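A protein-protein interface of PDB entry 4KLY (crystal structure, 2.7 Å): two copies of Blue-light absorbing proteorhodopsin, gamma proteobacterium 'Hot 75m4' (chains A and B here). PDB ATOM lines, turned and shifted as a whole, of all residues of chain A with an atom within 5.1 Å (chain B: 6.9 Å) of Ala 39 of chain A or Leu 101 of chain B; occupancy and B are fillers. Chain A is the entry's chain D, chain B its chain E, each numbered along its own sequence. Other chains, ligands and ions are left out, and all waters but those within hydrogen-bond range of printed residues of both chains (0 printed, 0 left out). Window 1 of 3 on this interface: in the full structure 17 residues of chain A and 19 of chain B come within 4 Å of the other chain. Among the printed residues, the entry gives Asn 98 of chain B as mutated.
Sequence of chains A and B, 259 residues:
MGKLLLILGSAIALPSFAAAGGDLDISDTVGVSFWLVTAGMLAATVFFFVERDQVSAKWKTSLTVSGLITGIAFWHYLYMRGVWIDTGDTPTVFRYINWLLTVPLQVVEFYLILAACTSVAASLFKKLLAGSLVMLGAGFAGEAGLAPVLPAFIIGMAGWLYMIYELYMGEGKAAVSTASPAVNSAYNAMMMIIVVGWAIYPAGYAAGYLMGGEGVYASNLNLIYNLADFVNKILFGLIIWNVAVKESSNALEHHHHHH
No position is printed for both chains. Of the 4 pairs that touch across the chains among the printed residues, none has its exchanged pair printed and touching as well.
The indole nitrogen (NE1) of Trp 35 of chain A is in hydrogen-bond range of a ring nitrogen (NE2) of His 76 of chain B.
Trp 35 of chain A touches Ile 97 of chain B (NE1 to CG2, 3.6 Å). CD2 of Leu 101 of chain B touches O of Leu 36 of chain A, at 3.96 Å. Ala 39 of chain A touches Leu 101 of chain B.
Of the 15 printed residues of chain B, 3 touch a printed residue of chain A. Hydrophobic or aromatic side chains of chain B within 4 Å of the printed part of chain A: His 76, Ile 97 and Leu 101. Among the printed residues, 4 pairs touch across the chains. Among the printed residues, no Asp or Glu carboxylate lies within 4 Å of a Lys or Arg side-chain nitrogen of the other chain.
Of the printed residues of chain B, Ala 39 of chain A touches Leu 101 (3.8 Å). Of the printed residues of chain A, Ile 97 of chain B touches Trp 35. Printed residues of chain B within 4 Å of Trp 35 of chain A: His 76 and Ile 97. Of the printed residues of chain B, Leu 36 of chain A touches Leu 101 (3.96 Å). Thr 102 of chain B touches none of the printed residues of chain A. Ile 69 of chain B touches none of the printed residues of chain A.
ND1 of His 76 of chain B sits at hydrogen-bond distance from O of Ile 72 of chain B (3.0 Å).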
ATOM      1  N   TRP A  35      28.433  -1.529 -27.001  1.00  0.00           N
ATOM      2  CA  TRP A  35      27.771  -0.412 -27.612  1.00  0.00           C
ATOM      3  C   TRP A  35      26.667   0.156 -26.678  1.00  0.00           C
ATOM      4  O   TRP A  35      26.637   1.354 -26.352  1.00  0.00           O
ATOM      5  CB  TRP A  35      27.165  -0.867 -28.924  1.00  0.00           C
ATOM      6  CG  TRP A  35      26.521   0.266 -29.608  1.00  0.00           C
ATOM      7  CD1 TRP A  35      25.314   0.790 -29.324  1.00  0.00           C
ATOM      8  CD2 TRP A  35      27.079   1.071 -30.653  1.00  0.00           C
ATOM      9  NE1 TRP A  35      25.083   1.869 -30.109  1.00  0.00           N
ATOM     10  CE2 TRP A  35      26.149   2.067 -30.937  1.00  0.00           C
ATOM     11  CE3 TRP A  35      28.290   1.044 -31.373  1.00  0.00           C
ATOM     12  CZ2 TRP A  35      26.371   3.035 -31.898  1.00  0.00           C
ATOM     13  CZ3 TRP A  35      28.510   2.002 -32.338  1.00  0.00           C
ATOM     14  CH2 TRP A  35      27.566   2.989 -32.586  1.00  0.00           C
ATOM     15  N   LEU A  36      25.756  -0.710 -26.266  1.00  0.00           N
ATOM     16  CA  LEU A  36      24.566  -0.321 -25.489  1.00  0.00           C
ATOM     17  C   LEU A  36      24.909   0.402 -24.185  1.00  0.00           C
ATOM     18  O   LEU A  36      24.286   1.419 -23.857  1.00  0.00           O
ATOM     19  CB  LEU A  36      23.723  -1.561 -25.142  1.00  0.00           C
ATOM     20  CG  LEU A  36      22.986  -2.228 -26.289  1.00  0.00           C
ATOM     21  CD1 LEU A  36      22.355  -3.543 -25.862  1.00  0.00           C
ATOM     22  CD2 LEU A  36      21.920  -1.311 -26.840  1.00  0.00           C
ATOM     23  N   VAL A  37      25.883  -0.152 -23.459  1.00  0.00           N
ATOM     24  CA  VAL A  37      26.364   0.402 -22.189  1.00  0.00           C
ATOM     25  C   VAL A  37      27.162   1.683 -22.405  1.00  0.00           C
ATOM     26  O   VAL A  37      27.026   2.644 -21.654  1.00  0.00           O
ATOM     27  CB  VAL A  37      27.224  -0.626 -21.441  1.00  0.00           C
ATOM     28  CG1 VAL A  37      27.965   0.006 -20.265  1.00  0.00           C
ATOM     29  CG2 VAL A  37      26.345  -1.787 -20.984  1.00  0.00           C
ATOM     30  N   THR A  38      27.964   1.729 -23.459  1.00  0.00           N
ATOM     31  CA  THR A  38      28.522   3.007 -23.857  1.00  0.00           C
ATOM     32  C   THR A  38      27.418   4.057 -23.840  1.00  0.00           C
ATOM     33  O   THR A  38      27.587   5.074 -23.209  1.00  0.00           O
ATOM     34  CB  THR A  38      29.118   2.999 -25.267  1.00  0.00           C
ATOM     35  OG1 THR A  38      30.097   1.974 -25.360  1.00  0.00           O
ATOM     36  CG2 THR A  38      29.765   4.317 -25.524  1.00  0.00           C
ATOM     37  N   ALA A  39      26.309   3.798 -24.550  1.00  0.00           N
ATOM     38  CA  ALA A  39      25.209   4.771 -24.701  1.00  0.00           C
ATOM     39  C   ALA A  39      24.539   5.004 -23.378  1.00  0.00           C
ATOM     40  O   ALA A  39      24.118   6.111 -23.058  1.00  0.00           O
ATOM     41  CB  ALA A  39      24.165   4.276 -25.692  1.00  0.00           C
ATOM     42  N   GLY A  40      24.428   3.924 -22.627  1.00  0.00           N
ATOM     43  CA  GLY A  40      23.769   3.959 -21.366  1.00  0.00           C
ATOM     44  C   GLY A  40      24.470   4.965 -20.523  1.00  0.00           C
ATOM     45  O   GLY A  40      23.823   5.746 -19.804  1.00  0.00           O
ATOM     46  N   MET A  41      25.785   4.976 -20.627  1.00  0.00           N
ATOM     47  CA  MET A  41      26.564   5.811 -19.721  1.00  0.00           C
ATOM     48  C   MET A  41      26.484   7.237 -20.175  1.00  0.00           C
ATOM     49  O   MET A  41      26.394   8.177 -19.391  1.00  0.00           O
ATOM     50  CB  MET A  41      28.027   5.421 -19.715  1.00  0.00           C
ATOM     51  CG  MET A  41      28.349   3.997 -19.273  1.00  0.00           C
ATOM     52  SD  MET A  41      28.179   3.862 -17.324  1.00  0.00           S
ATOM     53  CE  MET A  41      27.155   2.189 -17.357  1.00  0.00           C
ATOM     54  N   LEU A  42      26.532   7.432 -21.473  1.00  0.00           N
ATOM     55  CA  LEU A  42      26.450   8.774 -21.982  1.00  0.00           C
ATOM     56  C   LEU A  42      25.082   9.423 -21.647  1.00  0.00           C
ATOM     57  O   LEU A  42      25.028  10.554 -21.230  1.00  0.00           O
ATOM     58  CB  LEU A  42      26.743   8.786 -23.468  1.00  0.00           C
ATOM     59  CG  LEU A  42      26.438  10.140 -24.075  1.00  0.00           C
ATOM     60  CD1 LEU A  42      27.448  11.215 -23.637  1.00  0.00           C
ATOM     61  CD2 LEU A  42      26.324   9.991 -25.589  1.00  0.00           C
ATOM     62  N   ALA A  43      23.997   8.710 -21.877  1.00  0.00           N
ATOM     63  CA  ALA A  43      22.652   9.166 -21.477  1.00  0.00           C
ATOM     64  C   ALA A  43      22.704   9.521 -20.013  1.00  0.00           C
ATOM     65  O   ALA A  43      22.376  10.610 -19.624  1.00  0.00           O
ATOM     66  CB  ALA A  43      21.616   8.077 -21.718  1.00  0.00           C
ATOM     67  N   ALA A  44      23.197   8.580 -19.231  1.00  0.00           N
ATOM     68  CA  ALA A  44      23.271   8.701 -17.800  1.00  0.00           C
ATOM     69  C   ALA A  44      24.015   9.939 -17.359  1.00  0.00           C
ATOM     70  O   ALA A  44      23.533  10.711 -16.530  1.00  0.00           O
ATOM     71  CB  ALA A  44      23.961   7.463 -17.249  1.00  0.00           C
ATOM     72  N   ILE B  69      16.228  10.912 -25.462  1.00  0.00           N
ATOM     73  CA  ILE B  69      15.672  10.183 -26.619  1.00  0.00           C
ATOM     74  C   ILE B  69      16.248  10.731 -27.946  1.00  0.00           C
ATOM     75  O   ILE B  69      16.861   9.957 -28.748  1.00  0.00           O
ATOM     76  CB  ILE B  69      14.127  10.237 -26.643  1.00  0.00           C
ATOM     77  CG1 ILE B  69      13.512   9.386 -25.517  1.00  0.00           C
ATOM     78  CG2 ILE B  69      13.569   9.776 -27.958  1.00  0.00           C
ATOM     79  CD1 ILE B  69      12.201   9.952 -24.979  1.00  0.00           C
ATOM     80  N   ILE B  72      20.230  10.349 -28.230  1.00  0.00           N
ATOM     81  CA  ILE B  72      20.629   8.994 -28.602  1.00  0.00           C
ATOM     82  C   ILE B  72      20.356   8.713 -30.109  1.00  0.00           C
ATOM     83  O   ILE B  72      21.266   8.350 -30.892  1.00  0.00           O
ATOM     84  CB  ILE B  72      19.930   7.975 -27.690  1.00  0.00           C
ATOM     85  CG1 ILE B  72      20.509   8.065 -26.267  1.00  0.00           C
ATOM     86  CG2 ILE B  72      20.085   6.552 -28.232  1.00  0.00           C
ATOM     87  CD1 ILE B  72      19.526   7.621 -25.193  1.00  0.00           C
ATOM     88  N   HIS B  76      22.790   7.679 -33.238  1.00  0.00           N
ATOM     89  CA  HIS B  76      22.481   6.504 -34.084  1.00  0.00           C
ATOM     90  C   HIS B  76      22.169   6.810 -35.538  1.00  0.00           C
ATOM     91  O   HIS B  76      22.504   6.034 -36.388  1.00  0.00           O
ATOM     92  CB  HIS B  76      21.349   5.675 -33.466  1.00  0.00           C
ATOM     93  CG  HIS B  76      21.814   4.888 -32.297  1.00  0.00           C
ATOM     94  ND1 HIS B  76      21.993   5.451 -31.059  1.00  0.00           N
ATOM     95  CD2 HIS B  76      22.279   3.625 -32.208  1.00  0.00           C
ATOM     96  CE1 HIS B  76      22.489   4.551 -30.234  1.00  0.00           C
ATOM     97  NE2 HIS B  76      22.677   3.436 -30.909  1.00  0.00           N
ATOM     98  N   TYR B  96      17.360  -0.923 -34.643  1.00  0.00           N
ATOM     99  CA  TYR B  96      16.763  -1.621 -33.514  1.00  0.00           C
ATOM    100  C   TYR B  96      17.575  -1.354 -32.247  1.00  0.00           C
ATOM    101  O   TYR B  96      17.023  -1.252 -31.142  1.00  0.00           O
ATOM    102  CB  TYR B  96      16.582  -3.128 -33.792  1.00  0.00           C
ATOM    103  CG  TYR B  96      15.363  -3.416 -34.632  1.00  0.00           C
ATOM    104  CD1 TYR B  96      15.422  -3.351 -36.016  1.00  0.00           C
ATOM    105  CD2 TYR B  96      14.139  -3.723 -34.042  1.00  0.00           C
ATOM    106  CE1 TYR B  96      14.301  -3.587 -36.803  1.00  0.00           C
ATOM    107  CE2 TYR B  96      13.007  -3.968 -34.825  1.00  0.00           C
ATOM    108  CZ  TYR B  96      13.091  -3.896 -36.206  1.00  0.00           C
ATOM    109  OH  TYR B  96      11.966  -4.100 -36.994  1.00  0.00           O
ATOM    110  N   ILE B  97      18.879  -1.201 -32.371  1.00  0.00           N
ATOM    111  CA  ILE B  97      19.638  -0.776 -31.186  1.00  0.00           C
ATOM    112  C   ILE B  97      19.243   0.636 -30.653  1.00  0.00           C
ATOM    113  O   ILE B  97      19.180   0.841 -29.438  1.00  0.00           O
ATOM    114  CB  ILE B  97      21.145  -0.994 -31.399  1.00  0.00           C
ATOM    115  CG1 ILE B  97      21.462  -2.404 -30.927  1.00  0.00           C
ATOM    116  CG2 ILE B  97      21.989   0.026 -30.653  1.00  0.00           C
ATOM    117  CD1 ILE B  97      22.793  -2.903 -31.415  1.00  0.00           C
ATOM    118  N   ASN B  98      18.924   1.573 -31.543  1.00  0.00           N
ATOM    119  CA  ASN B  98      18.397   2.873 -31.146  1.00  0.00           C
ATOM    120  C   ASN B  98      17.087   2.720 -30.389  1.00  0.00           C
ATOM    121  O   ASN B  98      16.906   3.259 -29.291  1.00  0.00           O
ATOM    122  CB  ASN B  98      18.174   3.714 -32.401  1.00  0.00           C
ATOM    123  CG  ASN B  98      17.840   5.164 -32.107  1.00  0.00           C
ATOM    124  OD1 ASN B  98      18.410   5.799 -31.206  1.00  0.00           O
ATOM    125  ND2 ASN B  98      16.920   5.712 -32.892  1.00  0.00           N
ATOM    126  N   TRP B  99      16.183   1.940 -30.983  1.00  0.00           N
ATOM    127  CA  TRP B  99      14.857   1.668 -30.408  1.00  0.00           C
ATOM    128  C   TRP B  99      14.899   1.004 -29.044  1.00  0.00           C
ATOM    129  O   TRP B  99      14.160   1.396 -28.133  1.00  0.00           O
ATOM    130  CB  TRP B  99      14.048   0.836 -31.387  1.00  0.00           C
ATOM    131  CG  TRP B  99      13.642   1.618 -32.590  1.00  0.00           C
ATOM    132  CD1 TRP B  99      13.737   2.951 -32.752  1.00  0.00           C
ATOM    133  CD2 TRP B  99      13.004   1.118 -33.769  1.00  0.00           C
ATOM    134  NE1 TRP B  99      13.231   3.326 -33.968  1.00  0.00           N
ATOM    135  CE2 TRP B  99      12.775   2.216 -34.615  1.00  0.00           C
ATOM    136  CE3 TRP B  99      12.612  -0.154 -34.192  1.00  0.00           C
ATOM    137  CZ2 TRP B  99      12.178   2.090 -35.855  1.00  0.00           C
ATOM    138  CZ3 TRP B  99      12.022  -0.287 -35.420  1.00  0.00           C
ATOM    139  CH2 TRP B  99      11.807   0.827 -36.247  1.00  0.00           C
ATOM    140  N   LEU B 100      15.781   0.031 -28.887  1.00  0.00           N
ATOM    141  CA  LEU B 100      16.009  -0.593 -27.581  1.00  0.00           C
ATOM    142  C   LEU B 100      16.369   0.446 -26.543  1.00  0.00           C
ATOM    143  O   LEU B 100      15.932   0.312 -25.428  1.00  0.00           O
ATOM    144  CB  LEU B 100      17.138  -1.636 -27.641  1.00  0.00           C
ATOM    145  CG  LEU B 100      17.211  -2.705 -26.546  1.00  0.00           C
ATOM    146  CD1 LEU B 100      15.856  -3.359 -26.361  1.00  0.00           C
ATOM    147  CD2 LEU B 100      18.259  -3.756 -26.915  1.00  0.00           C
ATOM    148  N   LEU B 101      17.157   1.478 -26.907  1.00  0.00           N
ATOM    149  CA  LEU B 101      17.562   2.549 -25.942  1.00  0.00           C
ATOM    150  C   LEU B 101      16.455   3.585 -25.706  1.00  0.00           C
ATOM    151  O   LEU B 101      16.233   4.073 -24.582  1.00  0.00           O
ATOM    152  CB  LEU B 101      18.818   3.234 -26.426  1.00  0.00           C
ATOM    153  CG  LEU B 101      20.051   2.321 -26.348  1.00  0.00           C
ATOM    154  CD1 LEU B 101      21.152   2.621 -27.387  1.00  0.00           C
ATOM    155  CD2 LEU B 101      20.603   2.386 -24.935  1.00  0.00           C
ATOM    156  N   THR B 102      15.731   3.862 -26.781  1.00  0.00           N
ATOM    157  CA  THR B 102      14.812   4.946 -26.848  1.00  0.00           C
ATOM    158  C   THR B 102      13.432   4.605 -26.298  1.00  0.00           C
ATOM    159  O   THR B 102      12.816   5.402 -25.574  1.00  0.00           O
ATOM    160  CB  THR B 102      14.593   5.310 -28.312  1.00  0.00           C
ATOM    161  OG1 THR B 102      15.836   5.686 -28.926  1.00  0.00           O
ATOM    162  CG2 THR B 102      13.639   6.457 -28.366  1.00  0.00           C
ATOM    163  N   VAL B 103      12.936   3.430 -26.702  1.00  0.00           N
ATOM    164  CA  VAL B 103      11.583   3.019 -26.405  1.00  0.00           C
ATOM    165  C   VAL B 103      11.347   2.929 -24.906  1.00  0.00           C
ATOM    166  O   VAL B 103      10.386   3.517 -24.415  1.00  0.00           O
ATOM    167  CB  VAL B 103      11.216   1.696 -27.109  1.00  0.00           C
ATOM    168  CG1 VAL B 103       9.897   1.141 -26.564  1.00  0.00           C
ATOM    169  CG2 VAL B 103      11.121   1.909 -28.617  1.00  0.00           C
ATOM    170  N   PRO B 104      12.235   2.225 -24.169  1.00  0.00           N
ATOM    171  CA  PRO B 104      12.145   2.177 -22.714  1.00  0.00           C
ATOM    172  C   PRO B 104      12.090   3.565 -22.080  1.00  0.00           C
ATOM    173  O   PRO B 104      11.295   3.779 -21.173  1.00  0.00           O
ATOM    174  CB  PRO B 104      13.442   1.491 -22.325  1.00  0.00           C
ATOM    175  CG  PRO B 104      13.787   0.655 -23.486  1.00  0.00           C
ATOM    176  CD  PRO B 104      13.460   1.549 -24.633  1.00  0.00           C
ATOM    177  N   LEU B 105      12.939   4.477 -22.573  1.00  0.00           N
ATOM    178  CA  LEU B 105      12.904   5.906 -22.220  1.00  0.00           C
ATOM    179  C   LEU B 105      11.558   6.596 -22.507  1.00  0.00           C
ATOM    180  O   LEU B 105      11.065   7.383 -21.691  1.00  0.00           O
ATOM    181  CB  LEU B 105      14.038   6.663 -22.938  1.00  0.00           C
ATOM    182  CG  LEU B 105      15.436   6.516 -22.310  1.00  0.00           C
ATOM    183  CD1 LEU B 105      16.514   7.234 -23.126  1.00  0.00           C
ATOM    184  CD2 LEU B 105      15.420   7.019 -20.876  1.00  0.00           C
ATOM    185  N   GLN B 106      10.966   6.309 -23.656  1.00  0.00           N
ATOM    186  CA  GLN B 106       9.597   6.743 -23.946  1.00  0.00           C
ATOM    187  C   GLN B 106       8.616   6.119 -22.916  1.00  0.00           C
ATOM    188  O   GLN B 106       7.720   6.793 -22.422  1.00  0.00           O
ATOM    189  CB  GLN B 106       9.228   6.358 -25.385  1.00  0.00           C
ATOM    190  CG  GLN B 106       8.052   7.089 -26.018  1.00  0.00           C
ATOM    191  CD  GLN B 106       8.389   8.495 -26.481  1.00  0.00           C
ATOM    192  OE1 GLN B 106       8.901   8.698 -27.591  1.00  0.00           O
ATOM    193  NE2 GLN B 106       8.089   9.484 -25.637  1.00  0.00           N
ATOM    194  N   LEU B 136       9.778  -5.306 -30.028  1.00  0.00           N
ATOM    195  CA  LEU B 136      11.040  -5.036 -30.725  1.00  0.00           C
ATOM    196  C   LEU B 136      11.828  -6.296 -31.151  1.00  0.00           C
ATOM    197  O   LEU B 136      12.247  -6.382 -32.292  1.00  0.00           O
ATOM    198  CB  LEU B 136      11.940  -4.126 -29.883  1.00  0.00           C
ATOM    199  CG  LEU B 136      11.554  -2.650 -29.781  1.00  0.00           C
ATOM    200  CD1 LEU B 136      12.684  -1.925 -29.094  1.00  0.00           C
ATOM    201  CD2 LEU B 136      11.223  -1.995 -31.123  1.00  0.00           C
